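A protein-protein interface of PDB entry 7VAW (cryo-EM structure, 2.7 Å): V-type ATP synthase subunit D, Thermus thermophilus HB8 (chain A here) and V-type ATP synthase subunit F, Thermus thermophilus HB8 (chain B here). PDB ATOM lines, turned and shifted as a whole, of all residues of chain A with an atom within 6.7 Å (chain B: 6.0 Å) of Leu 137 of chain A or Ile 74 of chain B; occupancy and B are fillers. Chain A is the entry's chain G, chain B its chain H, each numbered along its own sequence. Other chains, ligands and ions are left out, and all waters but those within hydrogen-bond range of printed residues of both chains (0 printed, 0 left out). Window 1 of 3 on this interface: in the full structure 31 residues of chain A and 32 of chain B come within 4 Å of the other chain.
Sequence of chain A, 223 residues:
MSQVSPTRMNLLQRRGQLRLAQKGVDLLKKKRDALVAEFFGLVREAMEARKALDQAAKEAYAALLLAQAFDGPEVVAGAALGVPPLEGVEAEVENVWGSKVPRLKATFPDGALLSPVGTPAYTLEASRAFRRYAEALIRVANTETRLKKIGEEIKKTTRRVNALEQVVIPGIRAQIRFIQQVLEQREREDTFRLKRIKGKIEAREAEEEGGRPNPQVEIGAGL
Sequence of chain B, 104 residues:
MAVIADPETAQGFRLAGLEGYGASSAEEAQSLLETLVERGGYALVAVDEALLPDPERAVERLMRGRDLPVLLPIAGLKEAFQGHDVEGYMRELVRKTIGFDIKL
The backbone carbonyl oxygen (O) of Ile 74 of chain B lies within hydrogen-bond range of the backbone NH (N) of Glu 49 of chain B. The backbone NH (N) of Leu 104 of chain A is in hydrogen-bond range of the side-chain amide oxygen (OD1) of Asn 142 of chain A (2.8 Å). O of Leu 72 of chain B sits at hydrogen-bond distance from N of Val 47 of chain B (3.4 Å). The backbone carbonyl oxygen of Val 47 of chain B lies within hydrogen-bond range of the backbone NH of Ile 74 of chain B (2.8 Å).
Among the printed residues, pairs that only touch across the chains: Arg 50 of chain A with Pro 73 of chain B (3.6 Å), Arg 50 of chain A with His 84 of chain B (3.6 Å), Leu 104 of chain A with Leu 44 of chain B (3.8 Å), Tyr 133 of chain A with Phe 13 of chain B (3.3 Å), Leu 137 of chain A with Ala 46 of chain B (3.8 Å), Leu 137 of chain A with Leu 72 of chain B (3.8 Å), Leu 137 of chain A with Ile 74 of chain B (3.5 Å) and Val 140 of chain A with Leu 72 of chain B (3.8 Å).
Printed residues of chain B within 4 Å of Tyr 133 of chain A: Phe 13 (3.3 Å). Leu 137 of chain A touches three residues of chain B. Printed residues of chain A within 4 Å of Ala 46 of chain B: Leu 137 (3.8 Å). The nearest residue of chain B that does not touch Leu 137 of chain A is Phe 13 of chain B (4.5 Å). The nearest printed residue of chain B that does not touch Arg 50 of chain A is Glu 49 of chain B (4.3 Å).
Of the 18 printed residues of chain B, 7 touch a printed residue of chain A. Printed residues of chain B that touch a printed residue of chain A: Phe 13, Leu 44, Ala 46, Leu 72, Pro 73, Ile 74 and His 84. Of the 15 printed residues of chain A, 5 touch a printed residue of chain B. Among the printed residues, 8 pairs touch across the chains.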
ATOM      1  N   ARG A  50     -24.505   6.018  20.444  1.00  0.00           N
ATOM      2  CA  ARG A  50     -23.755   7.238  20.722  1.00  0.00           C
ATOM      3  C   ARG A  50     -24.205   7.885  22.026  1.00  0.00           C
ATOM      4  O   ARG A  50     -23.379   8.419  22.775  1.00  0.00           O
ATOM      5  CB  ARG A  50     -23.890   8.208  19.551  1.00  0.00           C
ATOM      6  CG  ARG A  50     -23.189   9.535  19.753  1.00  0.00           C
ATOM      7  CD  ARG A  50     -21.679   9.384  19.702  1.00  0.00           C
ATOM      8  NE  ARG A  50     -21.198   9.053  18.367  1.00  0.00           N
ATOM      9  CZ  ARG A  50     -19.923   8.854  18.062  1.00  0.00           C
ATOM     10  NH1 ARG A  50     -18.969   8.970  18.971  1.00  0.00           N
ATOM     11  NH2 ARG A  50     -19.596   8.534  16.815  1.00  0.00           N
ATOM     12  N   LEU A  53     -22.613   5.924  24.712  1.00  0.00           N
ATOM     13  CA  LEU A  53     -21.213   6.324  24.789  1.00  0.00           C
ATOM     14  C   LEU A  53     -21.055   7.650  25.517  1.00  0.00           C
ATOM     15  O   LEU A  53     -20.097   7.838  26.274  1.00  0.00           O
ATOM     16  CB  LEU A  53     -20.614   6.422  23.390  1.00  0.00           C
ATOM     17  CG  LEU A  53     -19.113   6.707  23.396  1.00  0.00           C
ATOM     18  CD1 LEU A  53     -18.382   5.500  23.924  1.00  0.00           C
ATOM     19  CD2 LEU A  53     -18.615   7.080  22.012  1.00  0.00           C
ATOM     20  N   ALA A  56     -21.326   6.914  29.188  1.00  0.00           N
ATOM     21  CA  ALA A  56     -20.150   6.193  29.662  1.00  0.00           C
ATOM     22  C   ALA A  56     -18.943   7.117  29.783  1.00  0.00           C
ATOM     23  O   ALA A  56     -18.199   7.047  30.767  1.00  0.00           O
ATOM     24  CB  ALA A  56     -19.838   5.024  28.730  1.00  0.00           C
ATOM     25  N   LEU A 104     -15.741  -5.443  15.599  1.00  0.00           N
ATOM     26  CA  LEU A 104     -14.811  -5.509  16.715  1.00  0.00           C
ATOM     27  C   LEU A 104     -15.421  -6.230  17.912  1.00  0.00           C
ATOM     28  O   LEU A 104     -16.620  -6.126  18.189  1.00  0.00           O
ATOM     29  CB  LEU A 104     -14.373  -4.106  17.134  1.00  0.00           C
ATOM     30  CG  LEU A 104     -13.652  -3.285  16.068  1.00  0.00           C
ATOM     31  CD1 LEU A 104     -13.672  -1.816  16.442  1.00  0.00           C
ATOM     32  CD2 LEU A 104     -12.228  -3.777  15.878  1.00  0.00           C
ATOM     33  N   ARG A 132     -16.066  -0.395  30.832  1.00  0.00           N
ATOM     34  CA  ARG A 132     -17.366  -0.378  30.174  1.00  0.00           C
ATOM     35  C   ARG A 132     -17.464   0.765  29.168  1.00  0.00           C
ATOM     36  O   ARG A 132     -18.136   0.625  28.139  1.00  0.00           O
ATOM     37  CB  ARG A 132     -18.488  -0.322  31.213  1.00  0.00           C
ATOM     38  CG  ARG A 132     -18.825   1.045  31.757  1.00  0.00           C
ATOM     39  CD  ARG A 132     -19.823   0.912  32.894  1.00  0.00           C
ATOM     40  NE  ARG A 132     -20.621   2.118  33.072  1.00  0.00           N
ATOM     41  CZ  ARG A 132     -21.825   2.306  32.552  1.00  0.00           C
ATOM     42  NH1 ARG A 132     -22.405   1.384  31.799  1.00  0.00           N
ATOM     43  NH2 ARG A 132     -22.464   3.447  32.788  1.00  0.00           N
ATOM     44  N   TYR A 133     -16.771   1.878  29.419  1.00  0.00           N
ATOM     45  CA  TYR A 133     -16.705   2.956  28.442  1.00  0.00           C
ATOM     46  C   TYR A 133     -16.018   2.498  27.160  1.00  0.00           C
ATOM     47  O   TYR A 133     -16.479   2.803  26.055  1.00  0.00           O
ATOM     48  CB  TYR A 133     -15.978   4.149  29.063  1.00  0.00           C
ATOM     49  CG  TYR A 133     -15.662   5.291  28.127  1.00  0.00           C
ATOM     50  CD1 TYR A 133     -16.577   5.722  27.180  1.00  0.00           C
ATOM     51  CD2 TYR A 133     -14.445   5.949  28.205  1.00  0.00           C
ATOM     52  CE1 TYR A 133     -16.282   6.771  26.330  1.00  0.00           C
ATOM     53  CE2 TYR A 133     -14.144   6.997  27.365  1.00  0.00           C
ATOM     54  CZ  TYR A 133     -15.063   7.404  26.429  1.00  0.00           C
ATOM     55  OH  TYR A 133     -14.758   8.452  25.589  1.00  0.00           O
ATOM     56  N   ALA A 134     -14.919   1.752  27.288  1.00  0.00           N
ATOM     57  CA  ALA A 134     -14.213   1.259  26.112  1.00  0.00           C
ATOM     58  C   ALA A 134     -15.064   0.272  25.324  1.00  0.00           C
ATOM     59  O   ALA A 134     -15.090   0.310  24.087  1.00  0.00           O
ATOM     60  CB  ALA A 134     -12.889   0.616  26.525  1.00  0.00           C
ATOM     61  N   GLU A 135     -15.772  -0.625  26.018  1.00  0.00           N
ATOM     62  CA  GLU A 135     -16.598  -1.574  25.273  1.00  0.00           C
ATOM     63  C   GLU A 135     -17.804  -0.888  24.632  1.00  0.00           C
ATOM     64  O   GLU A 135     -18.216  -1.265  23.526  1.00  0.00           O
ATOM     65  CB  GLU A 135     -17.031  -2.740  26.163  1.00  0.00           C
ATOM     66  CG  GLU A 135     -17.858  -2.377  27.369  1.00  0.00           C
ATOM     67  CD  GLU A 135     -18.307  -3.600  28.145  1.00  0.00           C
ATOM     68  OE1 GLU A 135     -18.870  -4.523  27.521  1.00  0.00           O
ATOM     69  OE2 GLU A 135     -18.092  -3.643  29.375  1.00  0.00           O
ATOM     70  N   ALA A 136     -18.362   0.138  25.282  1.00  0.00           N
ATOM     71  CA  ALA A 136     -19.400   0.935  24.635  1.00  0.00           C
ATOM     72  C   ALA A 136     -18.850   1.662  23.415  1.00  0.00           C
ATOM     73  O   ALA A 136     -19.549   1.824  22.407  1.00  0.00           O
ATOM     74  CB  ALA A 136     -19.997   1.928  25.630  1.00  0.00           C
ATOM     75  N   LEU A 137     -17.596   2.112  23.489  1.00  0.00           N
ATOM     76  CA  LEU A 137     -16.962   2.737  22.334  1.00  0.00           C
ATOM     77  C   LEU A 137     -16.798   1.743  21.192  1.00  0.00           C
ATOM     78  O   LEU A 137     -16.958   2.098  20.020  1.00  0.00           O
ATOM     79  CB  LEU A 137     -15.612   3.327  22.739  1.00  0.00           C
ATOM     80  CG  LEU A 137     -14.778   3.921  21.607  1.00  0.00           C
ATOM     81  CD1 LEU A 137     -15.585   4.972  20.873  1.00  0.00           C
ATOM     82  CD2 LEU A 137     -13.490   4.512  22.146  1.00  0.00           C
ATOM     83  N   ILE A 138     -16.466   0.493  21.516  1.00  0.00           N
ATOM     84  CA  ILE A 138     -16.377  -0.538  20.485  1.00  0.00           C
ATOM     85  C   ILE A 138     -17.747  -0.791  19.861  1.00  0.00           C
ATOM     86  O   ILE A 138     -17.867  -0.983  18.642  1.00  0.00           O
ATOM     87  CB  ILE A 138     -15.760  -1.823  21.070  1.00  0.00           C
ATOM     88  CG1 ILE A 138     -14.234  -1.712  21.060  1.00  0.00           C
ATOM     89  CG2 ILE A 138     -16.224  -3.053  20.302  1.00  0.00           C
ATOM     90  CD1 ILE A 138     -13.540  -2.731  21.922  1.00  0.00           C
ATOM     91  N   ARG A 139     -18.799  -0.787  20.681  1.00  0.00           N
ATOM     92  CA  ARG A 139     -20.157  -0.887  20.146  1.00  0.00           C
ATOM     93  C   ARG A 139     -20.453   0.256  19.182  1.00  0.00           C
ATOM     94  O   ARG A 139     -21.008   0.047  18.093  1.00  0.00           O
ATOM     95  CB  ARG A 139     -21.172  -0.893  21.288  1.00  0.00           C
ATOM     96  CG  ARG A 139     -22.617  -0.927  20.823  1.00  0.00           C
ATOM     97  CD  ARG A 139     -23.565  -0.565  21.951  1.00  0.00           C
ATOM     98  NE  ARG A 139     -24.931  -0.368  21.480  1.00  0.00           N
ATOM     99  CZ  ARG A 139     -25.898   0.187  22.199  1.00  0.00           C
ATOM    100  NH1 ARG A 139     -25.684   0.610  23.434  1.00  0.00           N
ATOM    101  NH2 ARG A 139     -27.108   0.320  21.666  1.00  0.00           N
ATOM    102  N   VAL A 140     -20.087   1.477  19.573  1.00  0.00           N
ATOM    103  CA  VAL A 140     -20.307   2.639  18.717  1.00  0.00           C
ATOM    104  C   VAL A 140     -19.546   2.483  17.409  1.00  0.00           C
ATOM    105  O   VAL A 140     -20.061   2.801  16.332  1.00  0.00           O
ATOM    106  CB  VAL A 140     -19.909   3.931  19.455  1.00  0.00           C
ATOM    107  CG1 VAL A 140     -19.676   5.065  18.468  1.00  0.00           C
ATOM    108  CG2 VAL A 140     -20.979   4.314  20.451  1.00  0.00           C
ATOM    109  N   ALA A 141     -18.308   1.991  17.483  1.00  0.00           N
ATOM    110  CA  ALA A 141     -17.512   1.789  16.277  1.00  0.00           C
ATOM    111  C   ALA A 141     -18.161   0.768  15.350  1.00  0.00           C
ATOM    112  O   ALA A 141     -18.162   0.944  14.127  1.00  0.00           O
ATOM    113  CB  ALA A 141     -16.097   1.350  16.649  1.00  0.00           C
ATOM    114  N   ASN A 142     -18.701  -0.315  15.915  1.00  0.00           N
ATOM    115  CA  ASN A 142     -19.387  -1.305  15.088  1.00  0.00           C
ATOM    116  C   ASN A 142     -20.599  -0.696  14.394  1.00  0.00           C
ATOM    117  O   ASN A 142     -20.815  -0.904  13.189  1.00  0.00           O
ATOM    118  CB  ASN A 142     -19.808  -2.501  15.940  1.00  0.00           C
ATOM    119  CG  ASN A 142     -18.672  -3.463  16.196  1.00  0.00           C
ATOM    120  OD1 ASN A 142     -17.617  -3.375  15.569  1.00  0.00           O
ATOM    121  ND2 ASN A 142     -18.881  -4.392  17.118  1.00  0.00           N
ATOM    122  N   VAL B   3      -6.231   5.274  21.827  1.00  0.00           N
ATOM    123  CA  VAL B   3      -7.018   6.493  21.971  1.00  0.00           C
ATOM    124  C   VAL B   3      -6.089   7.694  21.869  1.00  0.00           C
ATOM    125  O   VAL B   3      -5.018   7.709  22.486  1.00  0.00           O
ATOM    126  CB  VAL B   3      -7.793   6.525  23.302  1.00  0.00           C
ATOM    127  CG1 VAL B   3      -8.570   7.826  23.429  1.00  0.00           C
ATOM    128  CG2 VAL B   3      -8.733   5.334  23.401  1.00  0.00           C
ATOM    129  N   ILE B   4      -6.500   8.697  21.098  1.00  0.00           N
ATOM    130  CA  ILE B   4      -5.765   9.949  20.954  1.00  0.00           C
ATOM    131  C   ILE B   4      -6.652  11.064  21.489  1.00  0.00           C
ATOM    132  O   ILE B   4      -7.698  11.372  20.903  1.00  0.00           O
ATOM    133  CB  ILE B   4      -5.363  10.217  19.500  1.00  0.00           C
ATOM    134  CG1 ILE B   4      -4.659   8.994  18.910  1.00  0.00           C
ATOM    135  CG2 ILE B   4      -4.475  11.442  19.415  1.00  0.00           C
ATOM    136  CD1 ILE B   4      -4.424   9.094  17.427  1.00  0.00           C
ATOM    137  N   ALA B   5      -6.235  11.673  22.593  1.00  0.00           N
ATOM    138  CA  ALA B   5      -6.995  12.738  23.233  1.00  0.00           C
ATOM    139  C   ALA B   5      -6.033  13.537  24.109  1.00  0.00           C
ATOM    140  O   ALA B   5      -4.810  13.428  23.962  1.00  0.00           O
ATOM    141  CB  ALA B   5      -8.183  12.157  24.017  1.00  0.00           C
ATOM    142  N   THR B   9      -7.225  12.083  29.327  1.00  0.00           N
ATOM    143  CA  THR B   9      -7.982  10.969  28.762  1.00  0.00           C
ATOM    144  C   THR B   9      -7.065   9.815  28.379  1.00  0.00           C
ATOM    145  O   THR B   9      -7.433   8.644  28.533  1.00  0.00           O
ATOM    146  CB  THR B   9      -8.788  11.440  27.552  1.00  0.00           C
ATOM    147  OG1 THR B   9      -9.576  12.580  27.915  1.00  0.00           O
ATOM    148  CG2 THR B   9      -9.714  10.335  27.060  1.00  0.00           C
ATOM    149  N   PHE B  13      -7.376   6.061  29.827  1.00  0.00           N
ATOM    150  CA  PHE B  13      -7.474   4.866  28.996  1.00  0.00           C
ATOM    151  C   PHE B  13      -6.349   3.885  29.303  1.00  0.00           C
ATOM    152  O   PHE B  13      -6.561   2.667  29.287  1.00  0.00           O
ATOM    153  CB  PHE B  13      -7.478   5.251  27.519  1.00  0.00           C
ATOM    154  CG  PHE B  13      -8.855   5.424  26.952  1.00  0.00           C
ATOM    155  CD1 PHE B  13      -9.654   4.322  26.702  1.00  0.00           C
ATOM    156  CD2 PHE B  13      -9.359   6.686  26.686  1.00  0.00           C
ATOM    157  CE1 PHE B  13     -10.925   4.473  26.187  1.00  0.00           C
ATOM    158  CE2 PHE B  13     -10.630   6.844  26.171  1.00  0.00           C
ATOM    159  CZ  PHE B  13     -11.412   5.736  25.920  1.00  0.00           C
ATOM    160  N   LEU B  44      -8.372  -0.594  16.609  1.00  0.00           N
ATOM    161  CA  LEU B  44      -9.224   0.587  16.632  1.00  0.00           C
ATOM    162  C   LEU B  44      -8.470   1.745  17.266  1.00  0.00           C
ATOM    163  O   LEU B  44      -7.810   1.570  18.295  1.00  0.00           O
ATOM    164  CB  LEU B  44     -10.523   0.312  17.399  1.00  0.00           C
ATOM    165  CG  LEU B  44     -11.391   1.510  17.778  1.00  0.00           C
ATOM    166  CD1 LEU B  44     -11.872   2.217  16.532  1.00  0.00           C
ATOM    167  CD2 LEU B  44     -12.565   1.069  18.638  1.00  0.00           C
ATOM    168  N   ALA B  46      -9.117   5.740  18.570  1.00  0.00           N
ATOM    169  CA  ALA B  46     -10.094   6.762  18.922  1.00  0.00           C
ATOM    170  C   ALA B  46      -9.399   8.112  19.007  1.00  0.00           C
ATOM    171  O   ALA B  46      -8.351   8.236  19.649  1.00  0.00           O
ATOM    172  CB  ALA B  46     -10.779   6.429  20.248  1.00  0.00           C
ATOM    173  N   VAL B  47      -9.981   9.119  18.361  1.00  0.00           N
ATOM    174  CA  VAL B  47      -9.397  10.453  18.288  1.00  0.00           C
ATOM    175  C   VAL B  47     -10.439  11.475  18.720  1.00  0.00           C
ATOM    176  O   VAL B  47     -11.610  11.388  18.334  1.00  0.00           O
ATOM    177  CB  VAL B  47      -8.865  10.761  16.871  1.00  0.00           C
ATOM    178  CG1 VAL B  47      -9.970  10.623  15.841  1.00  0.00           C
ATOM    179  CG2 VAL B  47      -8.242  12.149  16.820  1.00  0.00           C
ATOM    180  N   ASP B  48     -10.011  12.438  19.532  1.00  0.00           N
ATOM    181  CA  ASP B  48     -10.928  13.426  20.083  1.00  0.00           C
ATOM    182  C   ASP B  48     -11.524  14.297  18.983  1.00  0.00           C
ATOM    183  O   ASP B  48     -10.864  14.619  17.990  1.00  0.00           O
ATOM    184  CB  ASP B  48     -10.204  14.297  21.111  1.00  0.00           C
ATOM    185  CG  ASP B  48     -11.134  15.262  21.824  1.00  0.00           C
ATOM    186  OD1 ASP B  48     -12.360  15.204  21.592  1.00  0.00           O
ATOM    187  OD2 ASP B  48     -10.635  16.090  22.615  1.00  0.00           O
ATOM    188  N   GLU B  49     -12.790  14.681  19.172  1.00  0.00           N
ATOM    189  CA  GLU B  49     -13.461  15.552  18.213  1.00  0.00           C
ATOM    190  C   GLU B  49     -12.911  16.971  18.260  1.00  0.00           C
ATOM    191  O   GLU B  49     -12.727  17.597  17.210  1.00  0.00           O
ATOM    192  CB  GLU B  49     -14.964  15.566  18.480  1.00  0.00           C
ATOM    193  CG  GLU B  49     -15.720  14.418  17.844  1.00  0.00           C
ATOM    194  CD  GLU B  49     -17.052  14.169  18.513  1.00  0.00           C
ATOM    195  OE1 GLU B  49     -17.665  15.146  18.990  1.00  0.00           O
ATOM    196  OE2 GLU B  49     -17.485  12.999  18.565  1.00  0.00           O
ATOM    197  N   ALA B  50     -12.647  17.496  19.457  1.00  0.00           N
ATOM    198  CA  ALA B  50     -12.031  18.810  19.579  1.00  0.00           C
ATOM    199  C   ALA B  50     -10.576  18.806  19.136  1.00  0.00           C
ATOM    200  O   ALA B  50     -10.010  19.876  18.893  1.00  0.00           O
ATOM    201  CB  ALA B  50     -12.133  19.312  21.021  1.00  0.00           C
ATOM    202  N   LEU B  72     -12.444   6.295  14.456  1.00  0.00           N
ATOM    203  CA  LEU B  72     -13.656   7.098  14.561  1.00  0.00           C
ATOM    204  C   LEU B  72     -13.374   8.303  15.442  1.00  0.00           C
ATOM    205  O   LEU B  72     -12.477   8.248  16.291  1.00  0.00           O
ATOM    206  CB  LEU B  72     -14.826   6.297  15.154  1.00  0.00           C
ATOM    207  CG  LEU B  72     -14.831   6.092  16.674  1.00  0.00           C
ATOM    208  CD1 LEU B  72     -16.199   5.637  17.158  1.00  0.00           C
ATOM    209  CD2 LEU B  72     -13.760   5.123  17.125  1.00  0.00           C
ATOM    210  N   PRO B  73     -14.109   9.398  15.268  1.00  0.00           N
ATOM    211  CA  PRO B  73     -13.998  10.515  16.207  1.00  0.00           C
ATOM    212  C   PRO B  73     -14.777  10.251  17.486  1.00  0.00           C
ATOM    213  O   PRO B  73     -15.769   9.520  17.501  1.00  0.00           O
ATOM    214  CB  PRO B  73     -14.605  11.687  15.427  1.00  0.00           C
ATOM    215  CG  PRO B  73     -15.622  11.039  14.557  1.00  0.00           C
ATOM    216  CD  PRO B  73     -15.040   9.700  14.165  1.00  0.00           C
ATOM    217  N   ILE B  74     -14.308  10.866  18.571  1.00  0.00           N
ATOM    218  CA  ILE B  74     -14.951  10.756  19.875  1.00  0.00           C
ATOM    219  C   ILE B  74     -14.935  12.117  20.554  1.00  0.00           C
ATOM    220  O   ILE B  74     -14.059  12.950  20.299  1.00  0.00           O
ATOM    221  CB  ILE B  74     -14.270   9.706  20.780  1.00  0.00           C
ATOM    222  CG1 ILE B  74     -12.763   9.951  20.842  1.00  0.00           C
ATOM    223  CG2 ILE B  74     -14.564   8.306  20.286  1.00  0.00           C
ATOM    224  CD1 ILE B  74     -12.093   9.344  22.049  1.00  0.00           C
ATOM    225  N   ALA B  75     -15.914  12.340  21.424  1.00  0.00           N
ATOM    226  CA  ALA B  75     -15.946  13.564  22.212  1.00  0.00           C
ATOM    227  C   ALA B  75     -14.951  13.467  23.361  1.00  0.00           C
ATOM    228  O   ALA B  75     -14.958  12.496  24.122  1.00  0.00           O
ATOM    229  CB  ALA B  75     -17.354  13.816  22.747  1.00  0.00           C
ATOM    230  N   GLY B  76     -14.091  14.475  23.483  1.00  0.00           N
ATOM    231  CA  GLY B  76     -13.129  14.490  24.564  1.00  0.00           C
ATOM    232  C   GLY B  76     -13.795  14.631  25.917  1.00  0.00           C
ATOM    233  O   GLY B  76     -14.896  15.165  26.053  1.00  0.00           O
ATOM    234  N   GLU B  79     -15.315  18.083  27.078  1.00  0.00           N
ATOM    235  CA  GLU B  79     -16.638  18.427  26.572  1.00  0.00           C
ATOM    236  C   GLU B  79     -17.657  17.316  26.788  1.00  0.00           C
ATOM    237  O   GLU B  79     -18.860  17.597  26.815  1.00  0.00           O
ATOM    238  CB  GLU B  79     -16.562  18.786  25.085  1.00  0.00           C
ATOM    239  CG  GLU B  79     -16.160  17.642  24.174  1.00  0.00           C
ATOM    240  CD  GLU B  79     -14.657  17.542  23.990  1.00  0.00           C
ATOM    241  OE1 GLU B  79     -13.913  17.970  24.898  1.00  0.00           O
ATOM    242  OE2 GLU B  79     -14.221  17.038  22.934  1.00  0.00           O
ATOM    243  N   HIS B  84     -22.277  15.722  25.017  1.00  0.00           N
ATOM    244  CA  HIS B  84     -21.984  15.465  23.615  1.00  0.00           C
ATOM    245  C   HIS B  84     -23.222  15.704  22.758  1.00  0.00           C
ATOM    246  O   HIS B  84     -24.337  15.340  23.142  1.00  0.00           O
ATOM    247  CB  HIS B  84     -21.483  14.031  23.431  1.00  0.00           C
ATOM    248  CG  HIS B  84     -21.104  13.696  22.023  1.00  0.00           C
ATOM    249  ND1 HIS B  84     -20.542  14.614  21.163  1.00  0.00           N
ATOM    250  CD2 HIS B  84     -21.199  12.538  21.326  1.00  0.00           C
ATOM    251  CE1 HIS B  84     -20.311  14.039  19.996  1.00  0.00           C
ATOM    252  NE2 HIS B  84     -20.701  12.779  20.069  1.00  0.00           N
